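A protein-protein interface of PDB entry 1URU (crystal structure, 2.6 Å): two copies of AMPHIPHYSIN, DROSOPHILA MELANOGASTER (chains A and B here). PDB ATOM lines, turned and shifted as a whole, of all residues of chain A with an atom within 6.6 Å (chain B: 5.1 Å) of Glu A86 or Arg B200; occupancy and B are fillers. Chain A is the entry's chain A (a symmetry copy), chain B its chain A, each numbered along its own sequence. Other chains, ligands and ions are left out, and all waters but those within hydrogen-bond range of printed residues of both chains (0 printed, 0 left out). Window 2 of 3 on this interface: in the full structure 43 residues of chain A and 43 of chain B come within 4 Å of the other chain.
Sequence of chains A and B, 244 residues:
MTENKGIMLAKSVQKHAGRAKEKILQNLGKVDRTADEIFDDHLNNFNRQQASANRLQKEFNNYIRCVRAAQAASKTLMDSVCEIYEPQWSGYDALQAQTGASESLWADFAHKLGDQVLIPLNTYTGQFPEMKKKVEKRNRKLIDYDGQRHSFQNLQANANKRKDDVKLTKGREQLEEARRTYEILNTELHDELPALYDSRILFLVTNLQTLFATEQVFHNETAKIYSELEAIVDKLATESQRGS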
ATOM      1  N   VAL A  81       4.821  20.401   8.221  1.00  0.00           N
ATOM      2  CA  VAL A  81       4.009  21.058   7.225  1.00  0.00           C
ATOM      3  C   VAL A  81       4.041  22.548   7.543  1.00  0.00           C
ATOM      4  O   VAL A  81       4.157  23.374   6.637  1.00  0.00           O
ATOM      5  CB  VAL A  81       2.551  20.589   7.239  1.00  0.00           C
ATOM      6  CG1 VAL A  81       1.727  21.458   6.325  1.00  0.00           C
ATOM      7  CG2 VAL A  81       2.435  19.129   6.819  1.00  0.00           C
ATOM      8  N   CYS A  82       3.957  22.876   8.835  1.00  0.00           N
ATOM      9  CA  CYS A  82       3.991  24.263   9.276  1.00  0.00           C
ATOM     10  C   CYS A  82       5.357  24.875   8.956  1.00  0.00           C
ATOM     11  O   CYS A  82       5.414  26.008   8.506  1.00  0.00           O
ATOM     12  CB  CYS A  82       3.636  24.380  10.760  1.00  0.00           C
ATOM     13  SG  CYS A  82       1.856  24.175  11.136  1.00  0.00           S
ATOM     14  N   GLU A  83       6.446  24.120   9.122  1.00  0.00           N
ATOM     15  CA  GLU A  83       7.803  24.616   8.810  1.00  0.00           C
ATOM     16  C   GLU A  83       8.038  24.934   7.313  1.00  0.00           C
ATOM     17  O   GLU A  83       8.609  25.978   6.972  1.00  0.00           O
ATOM     18  CB  GLU A  83       8.874  23.612   9.289  1.00  0.00           C
ATOM     19  CG  GLU A  83      10.329  24.081   9.127  1.00  0.00           C
ATOM     20  CD  GLU A  83      11.043  23.512   7.873  1.00  0.00           C
ATOM     21  OE1 GLU A  83      10.943  24.138   6.782  1.00  0.00           O
ATOM     22  OE2 GLU A  83      11.719  22.447   7.969  1.00  0.00           O
ATOM     23  N   ILE A  84       7.619  24.021   6.437  1.00  0.00           N
ATOM     24  CA  ILE A  84       7.897  24.090   5.005  1.00  0.00           C
ATOM     25  C   ILE A  84       6.936  25.029   4.264  1.00  0.00           C
ATOM     26  O   ILE A  84       7.171  25.394   3.117  1.00  0.00           O
ATOM     27  CB  ILE A  84       7.825  22.657   4.406  1.00  0.00           C
ATOM     28  CG1 ILE A  84       8.400  22.631   2.992  1.00  0.00           C
ATOM     29  CG2 ILE A  84       6.377  22.117   4.399  1.00  0.00           C
ATOM     30  CD1 ILE A  84       8.847  21.274   2.551  1.00  0.00           C
ATOM     31  N   TYR A  85       5.836  25.368   4.926  1.00  0.00           N
ATOM     32  CA  TYR A  85       4.858  26.319   4.442  1.00  0.00           C
ATOM     33  C   TYR A  85       5.365  27.624   4.962  1.00  0.00           C
ATOM     34  O   TYR A  85       5.650  27.753   6.149  1.00  0.00           O
ATOM     35  CB  TYR A  85       3.514  26.013   5.069  1.00  0.00           C
ATOM     36  CG  TYR A  85       2.300  26.535   4.360  1.00  0.00           C
ATOM     37  CD1 TYR A  85       1.382  25.664   3.798  1.00  0.00           C
ATOM     38  CD2 TYR A  85       2.029  27.884   4.307  1.00  0.00           C
ATOM     39  CE1 TYR A  85       0.253  26.122   3.178  1.00  0.00           C
ATOM     40  CE2 TYR A  85       0.899  28.354   3.687  1.00  0.00           C
ATOM     41  CZ  TYR A  85       0.015  27.463   3.128  1.00  0.00           C
ATOM     42  OH  TYR A  85      -1.113  27.922   2.526  1.00  0.00           O
ATOM     43  N   GLU A  86       5.513  28.599   4.082  1.00  0.00           N
ATOM     44  CA  GLU A  86       6.239  29.805   4.435  1.00  0.00           C
ATOM     45  C   GLU A  86       5.313  30.925   4.912  1.00  0.00           C
ATOM     46  O   GLU A  86       4.151  31.001   4.485  1.00  0.00           O
ATOM     47  CB  GLU A  86       7.082  30.234   3.254  1.00  0.00           C
ATOM     48  CG  GLU A  86       7.916  29.074   2.737  1.00  0.00           C
ATOM     49  CD  GLU A  86       9.082  29.502   1.888  1.00  0.00           C
ATOM     50  OE1 GLU A  86       9.115  30.676   1.445  1.00  0.00           O
ATOM     51  OE2 GLU A  86       9.965  28.648   1.662  1.00  0.00           O
ATOM     52  N   PRO A  87       5.822  31.776   5.803  1.00  0.00           N
ATOM     53  CA  PRO A  87       5.038  32.889   6.363  1.00  0.00           C
ATOM     54  C   PRO A  87       4.375  33.768   5.300  1.00  0.00           C
ATOM     55  O   PRO A  87       3.216  34.150   5.403  1.00  0.00           O
ATOM     56  CB  PRO A  87       6.088  33.702   7.132  1.00  0.00           C
ATOM     57  CG  PRO A  87       7.191  32.755   7.430  1.00  0.00           C
ATOM     58  CD  PRO A  87       7.196  31.754   6.330  1.00  0.00           C
ATOM     59  N   GLN A  88       5.127  34.058   4.259  1.00  0.00           N
ATOM     60  CA  GLN A  88       4.685  34.985   3.241  1.00  0.00           C
ATOM     61  C   GLN A  88       3.582  34.434   2.307  1.00  0.00           C
ATOM     62  O   GLN A  88       2.977  35.203   1.554  1.00  0.00           O
ATOM     63  CB  GLN A  88       5.906  35.476   2.434  1.00  0.00           C
ATOM     64  CG  GLN A  88       6.287  34.622   1.235  1.00  0.00           C
ATOM     65  CD  GLN A  88       7.389  33.612   1.514  1.00  0.00           C
ATOM     66  OE1 GLN A  88       7.893  33.491   2.657  1.00  0.00           O
ATOM     67  NE2 GLN A  88       7.781  32.880   0.456  1.00  0.00           N
ATOM     68  N   TRP A  89       3.351  33.117   2.312  1.00  0.00           N
ATOM     69  CA  TRP A  89       2.282  32.522   1.492  1.00  0.00           C
ATOM     70  C   TRP A  89       0.942  32.772   2.150  1.00  0.00           C
ATOM     71  O   TRP A  89       0.861  32.973   3.362  1.00  0.00           O
ATOM     72  CB  TRP A  89       2.498  31.013   1.299  1.00  0.00           C
ATOM     73  CG  TRP A  89       3.799  30.661   0.625  1.00  0.00           C
ATOM     74  CD1 TRP A  89       4.660  31.520   0.042  1.00  0.00           C
ATOM     75  CD2 TRP A  89       4.380  29.362   0.487  1.00  0.00           C
ATOM     76  NE1 TRP A  89       5.756  30.853  -0.444  1.00  0.00           N
ATOM     77  CE2 TRP A  89       5.603  29.519  -0.193  1.00  0.00           C
ATOM     78  CE3 TRP A  89       3.998  28.077   0.877  1.00  0.00           C
ATOM     79  CZ2 TRP A  89       6.442  28.439  -0.496  1.00  0.00           C
ATOM     80  CZ3 TRP A  89       4.821  27.018   0.576  1.00  0.00           C
ATOM     81  CH2 TRP A  89       6.030  27.198  -0.093  1.00  0.00           C
ATOM     82  N   SER A  90      -0.120  32.778   1.361  1.00  0.00           N
ATOM     83  CA  SER A  90      -1.446  32.953   1.934  1.00  0.00           C
ATOM     84  C   SER A  90      -1.839  31.696   2.731  1.00  0.00           C
ATOM     85  O   SER A  90      -1.371  30.592   2.443  1.00  0.00           O
ATOM     86  CB  SER A  90      -2.483  33.294   0.854  1.00  0.00           C
ATOM     87  OG  SER A  90      -3.072  32.130   0.301  1.00  0.00           O
ATOM     88  N   GLY A  91      -2.686  31.890   3.738  1.00  0.00           N
ATOM     89  CA  GLY A  91      -3.118  30.828   4.626  1.00  0.00           C
ATOM     90  C   GLY A  91      -2.113  30.426   5.704  1.00  0.00           C
ATOM     91  O   GLY A  91      -2.367  29.484   6.444  1.00  0.00           O
ATOM     92  N   TYR A  92      -0.982  31.105   5.828  1.00  0.00           N
ATOM     93  CA  TYR A  92       0.046  30.592   6.724  1.00  0.00           C
ATOM     94  C   TYR A  92      -0.373  30.644   8.204  1.00  0.00           C
ATOM     95  O   TYR A  92      -0.148  29.690   8.937  1.00  0.00           O
ATOM     96  CB  TYR A  92       1.411  31.270   6.512  1.00  0.00           C
ATOM     97  CG  TYR A  92       2.422  30.847   7.555  1.00  0.00           C
ATOM     98  CD1 TYR A  92       3.168  29.677   7.412  1.00  0.00           C
ATOM     99  CD2 TYR A  92       2.604  31.599   8.719  1.00  0.00           C
ATOM    100  CE1 TYR A  92       4.080  29.288   8.392  1.00  0.00           C
ATOM    101  CE2 TYR A  92       3.512  31.218   9.695  1.00  0.00           C
ATOM    102  CZ  TYR A  92       4.239  30.070   9.528  1.00  0.00           C
ATOM    103  OH  TYR A  92       5.131  29.703  10.498  1.00  0.00           O
ATOM    104  N   LEU A  95      -2.919  28.213   8.954  1.00  0.00           N
ATOM    105  CA  LEU A  95      -2.395  26.855   8.998  1.00  0.00           C
ATOM    106  C   LEU A  95      -1.883  26.563  10.379  1.00  0.00           C
ATOM    107  O   LEU A  95      -2.232  25.535  10.961  1.00  0.00           O
ATOM    108  CB  LEU A  95      -1.253  26.683   8.004  1.00  0.00           C
ATOM    109  CG  LEU A  95      -0.545  25.335   7.964  1.00  0.00           C
ATOM    110  CD1 LEU A  95      -1.321  24.404   7.092  1.00  0.00           C
ATOM    111  CD2 LEU A  95       0.855  25.488   7.444  1.00  0.00           C
ATOM    112  N   ARG B  48      18.344  24.411   1.810  1.00  0.00           N
ATOM    113  CA  ARG B  48      17.175  24.568   2.683  1.00  0.00           C
ATOM    114  C   ARG B  48      15.941  23.862   2.137  1.00  0.00           C
ATOM    115  O   ARG B  48      15.124  23.346   2.906  1.00  0.00           O
ATOM    116  CB  ARG B  48      16.834  26.052   2.904  1.00  0.00           C
ATOM    117  CG  ARG B  48      17.564  26.716   4.090  1.00  0.00           C
ATOM    118  CD  ARG B  48      17.404  28.264   4.218  1.00  0.00           C
ATOM    119  NE  ARG B  48      16.832  28.872   3.009  1.00  0.00           N
ATOM    120  CZ  ARG B  48      15.536  29.073   2.779  1.00  0.00           C
ATOM    121  NH1 ARG B  48      14.618  28.740   3.685  1.00  0.00           N
ATOM    122  NH2 ARG B  48      15.151  29.598   1.625  1.00  0.00           N
ATOM    123  N   GLN B  49      15.797  23.867   0.813  1.00  0.00           N
ATOM    124  CA  GLN B  49      14.674  23.194   0.155  1.00  0.00           C
ATOM    125  C   GLN B  49      14.832  21.682   0.357  1.00  0.00           C
ATOM    126  O   GLN B  49      13.866  21.003   0.678  1.00  0.00           O
ATOM    127  CB  GLN B  49      14.614  23.552  -1.337  1.00  0.00           C
ATOM    128  CG  GLN B  49      13.416  23.002  -2.088  1.00  0.00           C
ATOM    129  CD  GLN B  49      13.421  23.334  -3.586  1.00  0.00           C
ATOM    130  OE1 GLN B  49      14.407  23.824  -4.120  1.00  0.00           O
ATOM    131  NE2 GLN B  49      12.310  23.075  -4.251  1.00  0.00           N
ATOM    132  N   TYR B 124       9.752  13.888  -5.561  1.00  0.00           N
ATOM    133  CA  TYR B 124      10.169  15.267  -5.432  1.00  0.00           C
ATOM    134  C   TYR B 124      11.403  15.320  -4.570  1.00  0.00           C
ATOM    135  O   TYR B 124      12.342  16.065  -4.846  1.00  0.00           O
ATOM    136  CB  TYR B 124       9.040  16.088  -4.812  1.00  0.00           C
ATOM    137  CG  TYR B 124       9.412  17.460  -4.300  1.00  0.00           C
ATOM    138  CD1 TYR B 124       9.524  18.562  -5.167  1.00  0.00           C
ATOM    139  CD2 TYR B 124       9.621  17.668  -2.940  1.00  0.00           C
ATOM    140  CE1 TYR B 124       9.863  19.836  -4.672  1.00  0.00           C
ATOM    141  CE2 TYR B 124       9.947  18.911  -2.442  1.00  0.00           C
ATOM    142  CZ  TYR B 124      10.057  19.998  -3.292  1.00  0.00           C
ATOM    143  OH  TYR B 124      10.350  21.227  -2.730  1.00  0.00           O
ATOM    144  N   LEU B 196      13.927  24.970  -9.815  1.00  0.00           N
ATOM    145  CA  LEU B 196      13.593  23.923  -8.838  1.00  0.00           C
ATOM    146  C   LEU B 196      13.050  24.499  -7.550  1.00  0.00           C
ATOM    147  O   LEU B 196      12.146  23.932  -6.935  1.00  0.00           O
ATOM    148  CB  LEU B 196      14.836  23.061  -8.513  1.00  0.00           C
ATOM    149  CG  LEU B 196      14.808  21.967  -7.406  1.00  0.00           C
ATOM    150  CD1 LEU B 196      13.644  20.968  -7.534  1.00  0.00           C
ATOM    151  CD2 LEU B 196      16.126  21.207  -7.400  1.00  0.00           C
ATOM    152  N   TYR B 197      13.623  25.614  -7.136  1.00  0.00           N
ATOM    153  CA  TYR B 197      13.169  26.320  -5.958  1.00  0.00           C
ATOM    154  C   TYR B 197      11.731  26.791  -6.109  1.00  0.00           C
ATOM    155  O   TYR B 197      10.964  26.761  -5.155  1.00  0.00           O
ATOM    156  CB  TYR B 197      14.088  27.517  -5.677  1.00  0.00           C
ATOM    157  CG  TYR B 197      13.869  28.106  -4.316  1.00  0.00           C
ATOM    158  CD1 TYR B 197      14.027  27.322  -3.166  1.00  0.00           C
ATOM    159  CD2 TYR B 197      13.464  29.426  -4.162  1.00  0.00           C
ATOM    160  CE1 TYR B 197      13.794  27.843  -1.894  1.00  0.00           C
ATOM    161  CE2 TYR B 197      13.241  29.965  -2.892  1.00  0.00           C
ATOM    162  CZ  TYR B 197      13.405  29.162  -1.762  1.00  0.00           C
ATOM    163  OH  TYR B 197      13.182  29.674  -0.506  1.00  0.00           O
ATOM    164  N   ASP B 198      11.361  27.216  -7.307  1.00  0.00           N
ATOM    165  CA  ASP B 198      10.012  27.715  -7.533  1.00  0.00           C
ATOM    166  C   ASP B 198       9.021  26.573  -7.583  1.00  0.00           C
ATOM    167  O   ASP B 198       7.926  26.701  -7.057  1.00  0.00           O
ATOM    168  CB  ASP B 198       9.955  28.573  -8.790  1.00  0.00           C
ATOM    169  CG  ASP B 198      10.742  29.867  -8.626  1.00  0.00           C
ATOM    170  OD1 ASP B 198      10.702  30.422  -7.490  1.00  0.00           O
ATOM    171  OD2 ASP B 198      11.433  30.388  -9.547  1.00  0.00           O
ATOM    172  N   SER B 199       9.414  25.444  -8.160  1.00  0.00           N
ATOM    173  CA  SER B 199       8.613  24.225  -8.080  1.00  0.00           C
ATOM    174  C   SER B 199       8.108  23.897  -6.668  1.00  0.00           C
ATOM    175  O   SER B 199       7.059  23.289  -6.534  1.00  0.00           O
ATOM    176  CB  SER B 199       9.384  23.026  -8.629  1.00  0.00           C
ATOM    177  OG  SER B 199      10.473  22.696  -7.792  1.00  0.00           O
ATOM    178  N   ARG B 200       8.823  24.329  -5.626  1.00  0.00           N
ATOM    179  CA  ARG B 200       8.443  24.029  -4.229  1.00  0.00           C
ATOM    180  C   ARG B 200       6.986  24.347  -3.866  1.00  0.00           C
ATOM    181  O   ARG B 200       6.381  23.616  -3.092  1.00  0.00           O
ATOM    182  CB  ARG B 200       9.416  24.688  -3.212  1.00  0.00           C
ATOM    183  CG  ARG B 200       8.975  26.030  -2.633  1.00  0.00           C
ATOM    184  CD  ARG B 200      10.078  26.891  -2.000  1.00  0.00           C
ATOM    185  NE  ARG B 200      10.254  28.112  -2.807  1.00  0.00           N
ATOM    186  CZ  ARG B 200       9.993  29.355  -2.406  1.00  0.00           C
ATOM    187  NH1 ARG B 200       9.595  29.619  -1.170  1.00  0.00           N
ATOM    188  NH2 ARG B 200      10.176  30.355  -3.255  1.00  0.00           N
ATOM    189  N   ILE B 201       6.441  25.438  -4.393  1.00  0.00           N
ATOM    190  CA  ILE B 201       5.104  25.886  -4.026  1.00  0.00           C
ATOM    191  C   ILE B 201       4.109  24.918  -4.620  1.00  0.00           C
ATOM    192  O   ILE B 201       3.301  24.344  -3.904  1.00  0.00           O
ATOM    193  CB  ILE B 201       4.795  27.310  -4.575  1.00  0.00           C
ATOM    194  CG1 ILE B 201       5.648  28.386  -3.899  1.00  0.00           C
ATOM    195  CG2 ILE B 201       3.303  27.662  -4.377  1.00  0.00           C
ATOM    196  CD1 ILE B 201       5.882  29.619  -4.786  1.00  0.00           C
ATOM    197  N   LEU B 202       4.172  24.748  -5.936  1.00  0.00           N
ATOM    198  CA  LEU B 202       3.263  23.856  -6.639  1.00  0.00           C
ATOM    199  C   LEU B 202       3.333  22.424  -6.091  1.00  0.00           C
ATOM    200  O   LEU B 202       2.310  21.750  -5.978  1.00  0.00           O
ATOM    201  CB  LEU B 202       3.545  23.852  -8.153  1.00  0.00           C
ATOM    202  CG  LEU B 202       2.676  22.905  -9.007  1.00  0.00           C
ATOM    203  CD1 LEU B 202       1.219  23.359  -9.043  1.00  0.00           C
ATOM    204  CD2 LEU B 202       3.254  22.755 -10.423  1.00  0.00           C
ATOM    205  N   PHE B 203       4.535  21.952  -5.769  1.00  0.00           N
ATOM    206  CA  PHE B 203       4.650  20.639  -5.193  1.00  0.00           C
ATOM    207  C   PHE B 203       3.831  20.529  -3.919  1.00  0.00           C
ATOM    208  O   PHE B 203       3.080  19.583  -3.740  1.00  0.00           O
ATOM    209  CB  PHE B 203       6.072  20.264  -4.842  1.00  0.00           C
ATOM    210  CG  PHE B 203       6.124  19.044  -3.979  1.00  0.00           C
ATOM    211  CD1 PHE B 203       5.715  17.815  -4.501  1.00  0.00           C
ATOM    212  CD2 PHE B 203       6.460  19.138  -2.639  1.00  0.00           C
ATOM    213  CE1 PHE B 203       5.706  16.680  -3.726  1.00  0.00           C
ATOM    214  CE2 PHE B 203       6.462  18.014  -1.846  1.00  0.00           C
ATOM    215  CZ  PHE B 203       6.072  16.772  -2.389  1.00  0.00           C
ATOM    216  N   LEU B 204       4.003  21.486  -3.021  1.00  0.00           N
ATOM    217  CA  LEU B 204       3.329  21.411  -1.728  1.00  0.00           C
ATOM    218  C   LEU B 204       1.833  21.634  -1.769  1.00  0.00           C
ATOM    219  O   LEU B 204       1.115  21.006  -1.011  1.00  0.00           O
ATOM    220  CB  LEU B 204       3.958  22.364  -0.724  1.00  0.00           C
ATOM    221  CG  LEU B 204       5.033  21.613   0.068  1.00  0.00           C
ATOM    222  CD1 LEU B 204       6.428  22.217  -0.153  1.00  0.00           C
ATOM    223  CD2 LEU B 204       4.629  21.583   1.538  1.00  0.00           C
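The guanidinium group (NH1) of Arg B200 lies within salt-bridge range of the side-chain carboxylate (OE1) of Glu A86 (2.9 Å).
The indole nitrogen (NE1) of Trp A89 sits close to the side-chain amide nitrogen (NE2) of Gln A88, 3.0 Å away. The backbone carbonyl oxygen of Tyr B197 sits at hydrogen-bond distance from the guanidinium group of Arg B200 (2.8 Å). OE1 of Glu A86 sits at hydrogen-bond distance from NE2 of Gln A88, 2.8 Å away.
Ile A84 touches Leu B204. Arg B200 touches Trp A89. Ile B201 touches Trp A89.
Of the printed residues of chain B, Glu A86 touches Arg B200 (2.9 Å). Arg B200 touches two residues of chain A. Of the printed residues of chain B, Ile A84 touches Leu B204. Of the printed residues of chain B, Trp A89 touches Arg B200 (3.4 Å) and Ile B201 (3.5 Å). Of the printed residues of chain A, Leu B204 touches Ile A84. The nearest printed residue of chain B that does not touch Glu A86 is Tyr B197 (4.01 Å). The nearest printed residue of chain A that does not touch Ile B201 is Gln A88 (6.5 Å).
Of the 12 printed residues of chain B, 3 touch a printed residue of chain A. Along chain B the printed residues that touch a printed residue of chain A span positions 200 to 204. Of the 13 printed residues of chain A, 3 touch a printed residue of chain B. Printed residues of chain A that touch a printed residue of chain B: Ile A84, Glu A86 and Trp A89. Among the printed residues, 4 pairs touch across the chains. Among the printed residues, Asp or Glu carboxylates within 4 Å of a Lys or Arg side-chain nitrogen of the other chain: Glu A86 with Arg B200 (2.9 Å).
No position is printed for both chains. Of the 4 pairs that touch across the chains among the printed residues, none has its exchanged pair printed and touching as well.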
